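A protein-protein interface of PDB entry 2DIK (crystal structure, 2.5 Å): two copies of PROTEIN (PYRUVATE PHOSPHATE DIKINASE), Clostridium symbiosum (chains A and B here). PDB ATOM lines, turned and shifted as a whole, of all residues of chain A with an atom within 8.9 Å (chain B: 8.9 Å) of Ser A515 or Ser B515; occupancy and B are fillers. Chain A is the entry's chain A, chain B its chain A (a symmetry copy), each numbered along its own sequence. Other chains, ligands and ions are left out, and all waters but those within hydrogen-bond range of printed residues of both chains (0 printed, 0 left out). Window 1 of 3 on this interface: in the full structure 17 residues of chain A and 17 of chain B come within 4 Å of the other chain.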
ATOM      1  N   GLN A 374      -0.721   2.993 -17.571  1.00  0.00           N
ATOM      2  CA  GLN A 374      -1.298   3.943 -18.488  1.00  0.00           C
ATOM      3  C   GLN A 374      -2.793   3.828 -18.687  1.00  0.00           C
ATOM      4  O   GLN A 374      -3.421   4.866 -18.854  1.00  0.00           O
ATOM      5  CB  GLN A 374      -0.645   3.888 -19.863  1.00  0.00           C
ATOM      6  CG  GLN A 374       0.741   4.548 -19.951  1.00  0.00           C
ATOM      7  CD  GLN A 374       1.284   4.391 -21.368  1.00  0.00           C
ATOM      8  OE1 GLN A 374       0.546   4.265 -22.386  1.00  0.00           O
ATOM      9  NE2 GLN A 374       2.601   4.266 -21.412  1.00  0.00           N
ATOM     10  N   LEU A 375      -3.315   2.575 -18.749  1.00  0.00           N
ATOM     11  CA  LEU A 375      -4.717   2.286 -19.010  1.00  0.00           C
ATOM     12  C   LEU A 375      -5.603   2.681 -17.869  1.00  0.00           C
ATOM     13  O   LEU A 375      -6.817   2.775 -18.094  1.00  0.00           O
ATOM     14  CB  LEU A 375      -5.050   0.798 -19.056  1.00  0.00           C
ATOM     15  CG  LEU A 375      -4.364  -0.090 -20.061  1.00  0.00           C
ATOM     16  CD1 LEU A 375      -4.946   0.132 -21.450  1.00  0.00           C
ATOM     17  CD2 LEU A 375      -2.876   0.150 -19.965  1.00  0.00           C
ATOM     18  N   LEU A 376      -5.033   2.693 -16.639  1.00  0.00           N
ATOM     19  CA  LEU A 376      -5.794   2.952 -15.430  1.00  0.00           C
ATOM     20  C   LEU A 376      -5.715   4.386 -15.007  1.00  0.00           C
ATOM     21  O   LEU A 376      -5.928   4.762 -13.858  1.00  0.00           O
ATOM     22  CB  LEU A 376      -5.527   1.950 -14.310  1.00  0.00           C
ATOM     23  CG  LEU A 376      -6.071   0.580 -14.716  1.00  0.00           C
ATOM     24  CD1 LEU A 376      -5.606  -0.546 -13.804  1.00  0.00           C
ATOM     25  CD2 LEU A 376      -7.589   0.623 -14.833  1.00  0.00           C
ATOM     26  N   HIS A 377      -5.332   5.181 -15.991  1.00  0.00           N
ATOM     27  CA  HIS A 377      -5.236   6.597 -15.801  1.00  0.00           C
ATOM     28  C   HIS A 377      -6.633   7.164 -15.872  1.00  0.00           C
ATOM     29  O   HIS A 377      -7.407   6.907 -16.831  1.00  0.00           O
ATOM     30  CB  HIS A 377      -4.344   7.335 -16.822  1.00  0.00           C
ATOM     31  CG  HIS A 377      -2.892   7.332 -16.480  1.00  0.00           C
ATOM     32  ND1 HIS A 377      -1.912   7.376 -17.486  1.00  0.00           N
ATOM     33  CD2 HIS A 377      -2.268   7.254 -15.266  1.00  0.00           C
ATOM     34  CE1 HIS A 377      -0.724   7.344 -16.867  1.00  0.00           C
ATOM     35  NE2 HIS A 377      -0.906   7.280 -15.532  1.00  0.00           N
ATOM     36  N   PRO A 378      -6.917   7.910 -14.795  1.00  0.00           N
ATOM     37  CA  PRO A 378      -8.159   8.634 -14.654  1.00  0.00           C
ATOM     38  C   PRO A 378      -8.447   9.343 -15.946  1.00  0.00           C
ATOM     39  O   PRO A 378      -7.655  10.190 -16.375  1.00  0.00           O
ATOM     40  CB  PRO A 378      -7.828   9.728 -13.627  1.00  0.00           C
ATOM     41  CG  PRO A 378      -6.508   9.361 -12.926  1.00  0.00           C
ATOM     42  CD  PRO A 378      -5.985   8.118 -13.620  1.00  0.00           C
ATOM     43  N   THR A 379      -9.544   9.015 -16.584  1.00  0.00           N
ATOM     44  CA  THR A 379      -9.808   9.739 -17.788  1.00  0.00           C
ATOM     45  C   THR A 379     -10.602  11.018 -17.507  1.00  0.00           C
ATOM     46  O   THR A 379     -10.658  11.543 -16.389  1.00  0.00           O
ATOM     47  CB  THR A 379     -10.485   8.866 -18.814  1.00  0.00           C
ATOM     48  OG1 THR A 379     -11.855   8.943 -18.568  1.00  0.00           O
ATOM     49  CG2 THR A 379     -10.023   7.450 -18.537  1.00  0.00           C
ATOM     50  N   GLN A 512     -11.761  10.884 -14.014  1.00  0.00           N
ATOM     51  CA  GLN A 512     -12.616   9.934 -13.372  1.00  0.00           C
ATOM     52  C   GLN A 512     -12.060   8.513 -13.166  1.00  0.00           C
ATOM     53  O   GLN A 512     -11.566   8.200 -12.068  1.00  0.00           O
ATOM     54  CB  GLN A 512     -14.043  10.015 -13.916  1.00  0.00           C
ATOM     55  CG  GLN A 512     -14.147   9.507 -15.352  1.00  0.00           C
ATOM     56  CD  GLN A 512     -15.594   9.311 -15.765  1.00  0.00           C
ATOM     57  OE1 GLN A 512     -15.991   8.350 -16.469  1.00  0.00           O
ATOM     58  NE2 GLN A 512     -16.404  10.275 -15.351  1.00  0.00           N
ATOM     59  N   GLU A 513     -12.166   7.636 -14.175  1.00  0.00           N
ATOM     60  CA  GLU A 513     -11.641   6.273 -14.033  1.00  0.00           C
ATOM     61  C   GLU A 513     -11.459   5.501 -15.352  1.00  0.00           C
ATOM     62  O   GLU A 513     -12.117   5.812 -16.354  1.00  0.00           O
ATOM     63  CB  GLU A 513     -12.361   5.425 -12.960  1.00  0.00           C
ATOM     64  CG  GLU A 513     -11.727   4.029 -12.771  1.00  0.00           C
ATOM     65  CD  GLU A 513     -12.354   3.222 -11.668  1.00  0.00           C
ATOM     66  OE1 GLU A 513     -12.164   3.452 -10.478  1.00  0.00           O
ATOM     67  OE2 GLU A 513     -13.144   2.288 -12.108  1.00  0.00           O
ATOM     68  N   ALA A 514     -10.591   4.470 -15.365  1.00  0.00           N
ATOM     69  CA  ALA A 514     -10.430   3.702 -16.581  1.00  0.00           C
ATOM     70  C   ALA A 514     -11.763   3.168 -17.163  1.00  0.00           C
ATOM     71  O   ALA A 514     -12.847   3.754 -16.998  1.00  0.00           O
ATOM     72  CB  ALA A 514      -9.432   2.574 -16.383  1.00  0.00           C
ATOM     73  N   SER A 515     -11.647   2.032 -17.860  1.00  0.00           N
ATOM     74  CA  SER A 515     -12.735   1.360 -18.549  1.00  0.00           C
ATOM     75  C   SER A 515     -12.129   0.547 -19.698  1.00  0.00           C
ATOM     76  O   SER A 515     -12.570   0.596 -20.854  1.00  0.00           O
ATOM     77  CB  SER A 515     -13.725   2.352 -19.155  1.00  0.00           C
ATOM     78  OG  SER A 515     -13.222   2.829 -20.394  1.00  0.00           O
ATOM     79  N   VAL A 516     -11.069  -0.150 -19.356  1.00  0.00           N
ATOM     80  CA  VAL A 516     -10.236  -0.948 -20.232  1.00  0.00           C
ATOM     81  C   VAL A 516     -10.829  -1.698 -21.437  1.00  0.00           C
ATOM     82  O   VAL A 516     -11.761  -2.497 -21.366  1.00  0.00           O
ATOM     83  CB  VAL A 516      -9.382  -1.820 -19.354  1.00  0.00           C
ATOM     84  CG1 VAL A 516      -8.524  -0.878 -18.491  1.00  0.00           C
ATOM     85  CG2 VAL A 516     -10.307  -2.657 -18.464  1.00  0.00           C
ATOM     86  N   SER A 517     -10.190  -1.448 -22.569  1.00  0.00           N
ATOM     87  CA  SER A 517     -10.509  -2.052 -23.827  1.00  0.00           C
ATOM     88  C   SER A 517     -10.580  -3.529 -23.658  1.00  0.00           C
ATOM     89  O   SER A 517     -10.128  -4.089 -22.676  1.00  0.00           O
ATOM     90  CB  SER A 517      -9.361  -1.815 -24.829  1.00  0.00           C
ATOM     91  OG  SER A 517      -8.364  -2.866 -24.754  1.00  0.00           O
ATOM     92  N   GLY A 518     -11.014  -4.177 -24.689  1.00  0.00           N
ATOM     93  CA  GLY A 518     -11.030  -5.615 -24.606  1.00  0.00           C
ATOM     94  C   GLY A 518      -9.685  -6.186 -25.020  1.00  0.00           C
ATOM     95  O   GLY A 518      -9.450  -7.420 -24.965  1.00  0.00           O
ATOM     96  N   SER A 519      -8.812  -5.293 -25.519  1.00  0.00           N
ATOM     97  CA  SER A 519      -7.524  -5.774 -25.995  1.00  0.00           C
ATOM     98  C   SER A 519      -6.737  -5.897 -24.761  1.00  0.00           C
ATOM     99  O   SER A 519      -5.943  -6.827 -24.547  1.00  0.00           O
ATOM    100  CB  SER A 519      -6.928  -5.000 -27.150  1.00  0.00           C
ATOM    101  OG  SER A 519      -7.589  -3.721 -27.213  1.00  0.00           O
ATOM    102  N   PHE A 520      -7.158  -5.037 -23.892  1.00  0.00           N
ATOM    103  CA  PHE A 520      -6.598  -5.141 -22.610  1.00  0.00           C
ATOM    104  C   PHE A 520      -6.984  -6.468 -21.988  1.00  0.00           C
ATOM    105  O   PHE A 520      -6.156  -7.178 -21.467  1.00  0.00           O
ATOM    106  CB  PHE A 520      -7.133  -4.046 -21.754  1.00  0.00           C
ATOM    107  CG  PHE A 520      -6.675  -4.213 -20.367  1.00  0.00           C
ATOM    108  CD1 PHE A 520      -7.429  -4.981 -19.494  1.00  0.00           C
ATOM    109  CD2 PHE A 520      -5.591  -3.504 -19.863  1.00  0.00           C
ATOM    110  CE1 PHE A 520      -7.081  -5.098 -18.149  1.00  0.00           C
ATOM    111  CE2 PHE A 520      -5.242  -3.623 -18.516  1.00  0.00           C
ATOM    112  CZ  PHE A 520      -5.971  -4.425 -17.644  1.00  0.00           C
ATOM    113  N   GLU A 521      -8.274  -6.789 -22.044  1.00  0.00           N
ATOM    114  CA  GLU A 521      -8.764  -8.015 -21.511  1.00  0.00           C
ATOM    115  C   GLU A 521      -8.272  -9.234 -22.235  1.00  0.00           C
ATOM    116  O   GLU A 521      -7.951 -10.224 -21.626  1.00  0.00           O
ATOM    117  CB  GLU A 521     -10.251  -8.003 -21.282  1.00  0.00           C
ATOM    118  CG  GLU A 521     -10.657  -6.877 -20.293  1.00  0.00           C
ATOM    119  CD  GLU A 521     -11.781  -7.304 -19.347  1.00  0.00           C
ATOM    120  OE1 GLU A 521     -11.985  -8.581 -19.451  1.00  0.00           O
ATOM    121  OE2 GLU A 521     -12.422  -6.577 -18.557  1.00  0.00           O
ATOM    122  N   LYS A 550     -11.758  -7.078  -9.352  1.00  0.00           N
ATOM    123  CA  LYS A 550     -12.196  -6.727 -10.664  1.00  0.00           C
ATOM    124  C   LYS A 550     -11.025  -6.624 -11.647  1.00  0.00           C
ATOM    125  O   LYS A 550     -11.191  -6.885 -12.866  1.00  0.00           O
ATOM    126  CB  LYS A 550     -12.980  -5.430 -10.556  1.00  0.00           C
ATOM    127  CG  LYS A 550     -13.355  -4.731 -11.867  1.00  0.00           C
ATOM    128  CD  LYS A 550     -14.263  -3.494 -11.675  1.00  0.00           C
ATOM    129  CE  LYS A 550     -15.670  -3.787 -11.080  1.00  0.00           C
ATOM    130  NZ  LYS A 550     -16.322  -2.658 -10.340  1.00  0.00           N
ATOM    131  N   LEU A 551      -9.829  -6.229 -11.145  1.00  0.00           N
ATOM    132  CA  LEU A 551      -8.673  -6.145 -12.030  1.00  0.00           C
ATOM    133  C   LEU A 551      -8.067  -7.510 -12.151  1.00  0.00           C
ATOM    134  O   LEU A 551      -7.185  -7.850 -12.974  1.00  0.00           O
ATOM    135  CB  LEU A 551      -7.689  -5.075 -11.620  1.00  0.00           C
ATOM    136  CG  LEU A 551      -8.398  -3.749 -11.659  1.00  0.00           C
ATOM    137  CD1 LEU A 551      -7.563  -2.628 -11.077  1.00  0.00           C
ATOM    138  CD2 LEU A 551      -8.868  -3.460 -13.094  1.00  0.00           C
ATOM    139  N   PHE A 856      -4.526  -1.232  -8.220  1.00  0.00           N
ATOM    140  CA  PHE A 856      -4.059  -0.861  -9.529  1.00  0.00           C
ATOM    141  C   PHE A 856      -2.853  -1.598 -10.106  1.00  0.00           C
ATOM    142  O   PHE A 856      -2.809  -1.806 -11.314  1.00  0.00           O
ATOM    143  CB  PHE A 856      -4.137   0.627  -9.834  1.00  0.00           C
ATOM    144  CG  PHE A 856      -5.555   1.119  -9.703  1.00  0.00           C
ATOM    145  CD1 PHE A 856      -6.609   0.340 -10.186  1.00  0.00           C
ATOM    146  CD2 PHE A 856      -5.888   2.280  -9.009  1.00  0.00           C
ATOM    147  CE1 PHE A 856      -7.947   0.707 -10.030  1.00  0.00           C
ATOM    148  CE2 PHE A 856      -7.217   2.705  -8.897  1.00  0.00           C
ATOM    149  CZ  PHE A 856      -8.255   1.907  -9.390  1.00  0.00           C
ATOM    150  N   GLN B 374     -28.145  -3.795 -24.528  1.00  0.00           N
ATOM    151  CA  GLN B 374     -27.953  -3.715 -23.102  1.00  0.00           C
ATOM    152  C   GLN B 374     -26.643  -3.103 -22.657  1.00  0.00           C
ATOM    153  O   GLN B 374     -26.657  -2.420 -21.641  1.00  0.00           O
ATOM    154  CB  GLN B 374     -28.079  -5.073 -22.424  1.00  0.00           C
ATOM    155  CG  GLN B 374     -29.519  -5.589 -22.264  1.00  0.00           C
ATOM    156  CD  GLN B 374     -29.491  -6.964 -21.604  1.00  0.00           C
ATOM    157  OE1 GLN B 374     -28.562  -7.349 -20.838  1.00  0.00           O
ATOM    158  NE2 GLN B 374     -30.464  -7.761 -22.016  1.00  0.00           N
ATOM    159  N   LEU B 375     -25.534  -3.425 -23.373  1.00  0.00           N
ATOM    160  CA  LEU B 375     -24.188  -2.984 -23.037  1.00  0.00           C
ATOM    161  C   LEU B 375     -23.997  -1.515 -23.258  1.00  0.00           C
ATOM    162  O   LEU B 375     -23.018  -0.980 -22.722  1.00  0.00           O
ATOM    163  CB  LEU B 375     -23.107  -3.502 -23.981  1.00  0.00           C
ATOM    164  CG  LEU B 375     -22.910  -4.986 -24.147  1.00  0.00           C
ATOM    165  CD1 LEU B 375     -22.195  -5.565 -22.934  1.00  0.00           C
ATOM    166  CD2 LEU B 375     -24.253  -5.613 -24.434  1.00  0.00           C
ATOM    167  N   LEU B 376     -24.786  -0.939 -24.198  1.00  0.00           N
ATOM    168  CA  LEU B 376     -24.640   0.450 -24.593  1.00  0.00           C
ATOM    169  C   LEU B 376     -25.589   1.350 -23.864  1.00  0.00           C
ATOM    170  O   LEU B 376     -25.927   2.453 -24.283  1.00  0.00           O
ATOM    171  CB  LEU B 376     -24.611   0.658 -26.105  1.00  0.00           C
ATOM    172  CG  LEU B 376     -23.329   0.050 -26.675  1.00  0.00           C
ATOM    173  CD1 LEU B 376     -23.336  -0.052 -28.194  1.00  0.00           C
ATOM    174  CD2 LEU B 376     -22.109   0.804 -26.165  1.00  0.00           C
ATOM    175  N   HIS B 377     -26.061   0.796 -22.761  1.00  0.00           N
ATOM    176  CA  HIS B 377     -26.952   1.512 -21.899  1.00  0.00           C
ATOM    177  C   HIS B 377     -26.123   2.467 -21.076  1.00  0.00           C
ATOM    178  O   HIS B 377     -25.111   2.086 -20.432  1.00  0.00           O
ATOM    179  CB  HIS B 377     -27.791   0.631 -20.948  1.00  0.00           C
ATOM    180  CG  HIS B 377     -29.040   0.092 -21.558  1.00  0.00           C
ATOM    181  ND1 HIS B 377     -29.580  -1.135 -21.136  1.00  0.00           N
ATOM    182  CD2 HIS B 377     -29.821   0.587 -22.566  1.00  0.00           C
ATOM    183  CE1 HIS B 377     -30.677  -1.348 -21.876  1.00  0.00           C
ATOM    184  NE2 HIS B 377     -30.852  -0.326 -22.738  1.00  0.00           N
ATOM    185  N   PRO B 378     -26.585   3.723 -21.165  1.00  0.00           N
ATOM    186  CA  PRO B 378     -26.020   4.817 -20.408  1.00  0.00           C
ATOM    187  C   PRO B 378     -25.829   4.366 -18.989  1.00  0.00           C
ATOM    188  O   PRO B 378     -26.805   4.011 -18.317  1.00  0.00           O
ATOM    189  CB  PRO B 378     -27.148   5.860 -20.381  1.00  0.00           C
ATOM    190  CG  PRO B 378     -28.192   5.485 -21.449  1.00  0.00           C
ATOM    191  CD  PRO B 378     -27.755   4.152 -22.025  1.00  0.00           C
ATOM    192  N   THR B 379     -24.605   4.356 -18.518  1.00  0.00           N
ATOM    193  CA  THR B 379     -24.465   3.962 -17.151  1.00  0.00           C
ATOM    194  C   THR B 379     -24.595   5.162 -16.209  1.00  0.00           C
ATOM    195  O   THR B 379     -25.131   6.225 -16.543  1.00  0.00           O
ATOM    196  CB  THR B 379     -23.180   3.205 -16.931  1.00  0.00           C
ATOM    197  OG1 THR B 379     -22.192   4.153 -16.670  1.00  0.00           O
ATOM    198  CG2 THR B 379     -22.859   2.520 -18.244  1.00  0.00           C
ATOM    199  N   GLN B 512     -24.526   8.221 -18.258  1.00  0.00           N
ATOM    200  CA  GLN B 512     -23.501   8.716 -19.125  1.00  0.00           C
ATOM    201  C   GLN B 512     -23.234   7.929 -20.421  1.00  0.00           C
ATOM    202  O   GLN B 512     -23.752   8.307 -21.487  1.00  0.00           O
ATOM    203  CB  GLN B 512     -22.260   9.133 -18.335  1.00  0.00           C
ATOM    204  CG  GLN B 512     -21.521   7.937 -17.740  1.00  0.00           C
ATOM    205  CD  GLN B 512     -20.149   8.335 -17.227  1.00  0.00           C
ATOM    206  OE1 GLN B 512     -19.127   7.617 -17.352  1.00  0.00           O
ATOM    207  NE2 GLN B 512     -20.132   9.497 -16.592  1.00  0.00           N
ATOM    208  N   GLU B 513     -22.408   6.873 -20.365  1.00  0.00           N
ATOM    209  CA  GLU B 513     -22.131   6.083 -21.570  1.00  0.00           C
ATOM    210  C   GLU B 513     -21.509   4.699 -21.316  1.00  0.00           C
ATOM    211  O   GLU B 513     -20.884   4.477 -20.269  1.00  0.00           O
ATOM    212  CB  GLU B 513     -21.383   6.859 -22.678  1.00  0.00           C
ATOM    213  CG  GLU B 513     -21.188   6.029 -23.966  1.00  0.00           C
ATOM    214  CD  GLU B 513     -20.545   6.794 -25.090  1.00  0.00           C
ATOM    215  OE1 GLU B 513     -21.137   7.644 -25.747  1.00  0.00           O
ATOM    216  OE2 GLU B 513     -19.293   6.489 -25.262  1.00  0.00           O
ATOM    217  N   ALA B 514     -21.643   3.761 -22.275  1.00  0.00           N
ATOM    218  CA  ALA B 514     -21.033   2.463 -22.078  1.00  0.00           C
ATOM    219  C   ALA B 514     -19.526   2.527 -21.728  1.00  0.00           C
ATOM    220  O   ALA B 514     -19.019   3.491 -21.128  1.00  0.00           O
ATOM    221  CB  ALA B 514     -21.275   1.563 -23.277  1.00  0.00           C
ATOM    222  N   SER B 515     -18.820   1.460 -22.118  1.00  0.00           N
ATOM    223  CA  SER B 515     -17.405   1.255 -21.862  1.00  0.00           C
ATOM    224  C   SER B 515     -17.145  -0.256 -21.860  1.00  0.00           C
ATOM    225  O   SER B 515     -16.512  -0.822 -20.960  1.00  0.00           O
ATOM    226  CB  SER B 515     -16.988   1.799 -20.499  1.00  0.00           C
ATOM    227  OG  SER B 515     -17.317   0.856 -19.490  1.00  0.00           O
ATOM    228  N   VAL B 516     -17.708  -0.894 -22.861  1.00  0.00           N
ATOM    229  CA  VAL B 516     -17.710  -2.325 -23.086  1.00  0.00           C
ATOM    230  C   VAL B 516     -16.511  -3.201 -22.683  1.00  0.00           C
ATOM    231  O   VAL B 516     -15.354  -3.005 -23.052  1.00  0.00           O
ATOM    232  CB  VAL B 516     -18.156  -2.548 -24.504  1.00  0.00           C
ATOM    233  CG1 VAL B 516     -19.578  -1.974 -24.618  1.00  0.00           C
ATOM    234  CG2 VAL B 516     -17.202  -1.787 -25.432  1.00  0.00           C
ATOM    235  N   SER B 517     -16.855  -4.241 -21.942  1.00  0.00           N
ATOM    236  CA  SER B 517     -15.939  -5.238 -21.473  1.00  0.00           C
ATOM    237  C   SER B 517     -15.131  -5.739 -22.619  1.00  0.00           C
ATOM    238  O   SER B 517     -15.452  -5.531 -23.774  1.00  0.00           O
ATOM    239  CB  SER B 517     -16.717  -6.466 -20.961  1.00  0.00           C
ATOM    240  OG  SER B 517     -16.968  -7.420 -22.025  1.00  0.00           O
ATOM    241  N   GLY B 518     -14.160  -6.530 -22.298  1.00  0.00           N
ATOM    242  CA  GLY B 518     -13.394  -7.104 -23.375  1.00  0.00           C
ATOM    243  C   GLY B 518     -14.051  -8.380 -23.872  1.00  0.00           C
ATOM    244  O   GLY B 518     -13.588  -9.019 -24.851  1.00  0.00           O
ATOM    245  N   SER B 519     -15.098  -8.809 -23.144  1.00  0.00           N
ATOM    246  CA  SER B 519     -15.741 -10.058 -23.522  1.00  0.00           C
ATOM    247  C   SER B 519     -16.632  -9.656 -24.617  1.00  0.00           C
ATOM    248  O   SER B 519     -16.821 -10.347 -25.632  1.00  0.00           O
ATOM    249  CB  SER B 519     -16.327 -10.858 -22.379  1.00  0.00           C
ATOM    250  OG  SER B 519     -16.471  -9.976 -21.250  1.00  0.00           O
ATOM    251  N   PHE B 520     -16.990  -8.424 -24.454  1.00  0.00           N
ATOM    252  CA  PHE B 520     -17.722  -7.857 -25.508  1.00  0.00           C
ATOM    253  C   PHE B 520     -16.864  -7.797 -26.756  1.00  0.00           C
ATOM    254  O   PHE B 520     -17.281  -8.189 -27.820  1.00  0.00           O
ATOM    255  CB  PHE B 520     -18.114  -6.469 -25.138  1.00  0.00           C
ATOM    256  CG  PHE B 520     -18.758  -5.800 -26.278  1.00  0.00           C
ATOM    257  CD1 PHE B 520     -17.975  -5.112 -27.190  1.00  0.00           C
ATOM    258  CD2 PHE B 520     -20.141  -5.708 -26.386  1.00  0.00           C
ATOM    259  CE1 PHE B 520     -18.547  -4.393 -28.238  1.00  0.00           C
ATOM    260  CE2 PHE B 520     -20.714  -4.987 -27.436  1.00  0.00           C
ATOM    261  CZ  PHE B 520     -19.932  -4.330 -28.379  1.00  0.00           C
ATOM    262  N   GLU B 521     -15.645  -7.286 -26.605  1.00  0.00           N
ATOM    263  CA  GLU B 521     -14.735  -7.189 -27.695  1.00  0.00           C
ATOM    264  C   GLU B 521     -14.278  -8.515 -28.228  1.00  0.00           C
ATOM    265  O   GLU B 521     -14.162  -8.695 -29.414  1.00  0.00           O
ATOM    266  CB  GLU B 521     -13.614  -6.217 -27.439  1.00  0.00           C
ATOM    267  CG  GLU B 521     -14.160  -4.789 -27.168  1.00  0.00           C
ATOM    268  CD  GLU B 521     -13.283  -3.699 -27.786  1.00  0.00           C
ATOM    269  OE1 GLU B 521     -12.404  -4.233 -28.576  1.00  0.00           O
ATOM    270  OE2 GLU B 521     -13.374  -2.465 -27.608  1.00  0.00           O
ATOM    271  N   LYS B 550     -16.084   3.527 -34.103  1.00  0.00           N
ATOM    272  CA  LYS B 550     -15.574   2.982 -32.887  1.00  0.00           C
ATOM    273  C   LYS B 550     -16.303   1.695 -32.488  1.00  0.00           C
ATOM    274  O   LYS B 550     -15.706   0.798 -31.840  1.00  0.00           O
ATOM    275  CB  LYS B 550     -15.676   4.061 -31.821  1.00  0.00           C
ATOM    276  CG  LYS B 550     -15.404   3.640 -30.374  1.00  0.00           C
ATOM    277  CD  LYS B 550     -15.397   4.819 -29.373  1.00  0.00           C
ATOM    278  CE  LYS B 550     -14.273   5.871 -29.594  1.00  0.00           C
ATOM    279  NZ  LYS B 550     -14.557   7.256 -29.093  1.00  0.00           N
ATOM    280  N   LEU B 551     -17.606   1.586 -32.849  1.00  0.00           N
ATOM    281  CA  LEU B 551     -18.339   0.367 -32.524  1.00  0.00           C
ATOM    282  C   LEU B 551     -18.055  -0.656 -33.581  1.00  0.00           C
ATOM    283  O   LEU B 551     -18.357  -1.870 -33.526  1.00  0.00           O
ATOM    284  CB  LEU B 551     -19.811   0.607 -32.287  1.00  0.00           C
ATOM    285  CG  LEU B 551     -19.949   1.554 -31.127  1.00  0.00           C
ATOM    286  CD1 LEU B 551     -21.376   2.020 -30.925  1.00  0.00           C
ATOM    287  CD2 LEU B 551     -19.348   0.912 -29.865  1.00  0.00           C
ATOM    288  N   PHE B 856     -25.316   3.046 -32.587  1.00  0.00           N
ATOM    289  CA  PHE B 856     -25.541   2.025 -31.599  1.00  0.00           C
ATOM    290  C   PHE B 856     -25.954   0.633 -32.072  1.00  0.00           C
ATOM    291  O   PHE B 856     -25.555  -0.345 -31.450  1.00  0.00           O
ATOM    292  CB  PHE B 856     -26.200   2.513 -30.318  1.00  0.00           C
ATOM    293  CG  PHE B 856     -25.366   3.592 -29.674  1.00  0.00           C
ATOM    294  CD1 PHE B 856     -23.976   3.467 -29.637  1.00  0.00           C
ATOM    295  CD2 PHE B 856     -25.911   4.786 -29.206  1.00  0.00           C
ATOM    296  CE1 PHE B 856     -23.146   4.464 -29.119  1.00  0.00           C
ATOM    297  CE2 PHE B 856     -25.108   5.771 -28.622  1.00  0.00           C
ATOM    298  CZ  PHE B 856     -23.718   5.623 -28.595  1.00  0.00           C
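Gln B512 touches its own counterpart, Gln A512.
Ser B515 touches its own counterpart, Ser A515.
Gly A518 touches its own counterpart, Gly B518.
Gly A518 touches Glu B521, and with the chains exchanged Glu A521 touches Gly B518.
Positions printed for both chains: 374, 375, 376, 377, 378, 379, 512, 513, 514, 515, 516, 517, 518, 519, 520, 521, 550, 551 and 856.
The side-chain amide oxygen (OE1) of Gln A512 lies close to the side-chain amide oxygen (OE1) of Gln B512, at 3.3 Å.
The backbone NH (N) of Gln A512 lies within hydrogen-bond range of the backbone carbonyl oxygen (O) of Thr A379 (2.7 Å).
The backbone carbonyl oxygen (O) of Thr B379 is in hydrogen-bond range of the backbone NH (N) of Gln B512.
Printed residues of chain B within 4 Å of Gln A512: Gln B512 (3.3 Å).
No residue of chain B comes within 4 Å of Ala A514.
Of the printed residues of chain B, Gly A518 touches Gly B518 and Glu B521.
Of the printed residues of chain A, Gln B512 touches Gln A512.
No residue of chain A comes within 4 Å of Ala B514.
Of chain A, only Ser A515 (3.6 Å) comes within 4 Å of Ser B515.
Printed residues of chain A within 4 Å of Gly B518: Gly A518 (3.1 Å) and Glu A521 (3.9 Å).
Printed residues of chain A within 4 Å of Glu B521: Gly A518 (3.9 Å).
The nearest residue of chain B that does not touch Ser A515 is Val B516 (5.1 Å).
Among the printed residues, merely in contact across the chains: Ser A515 with Ser B515 (3.6 Å), Gly A518 with Gly B518 (3.1 Å), Gly A518 with Glu B521 (3.9 Å) and Glu A521 with Gly B518 (3.9 Å).
Among the printed residues, no Asp or Glu carboxylate lies within 4 Å of a Lys or Arg side-chain nitrogen of the other chain.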
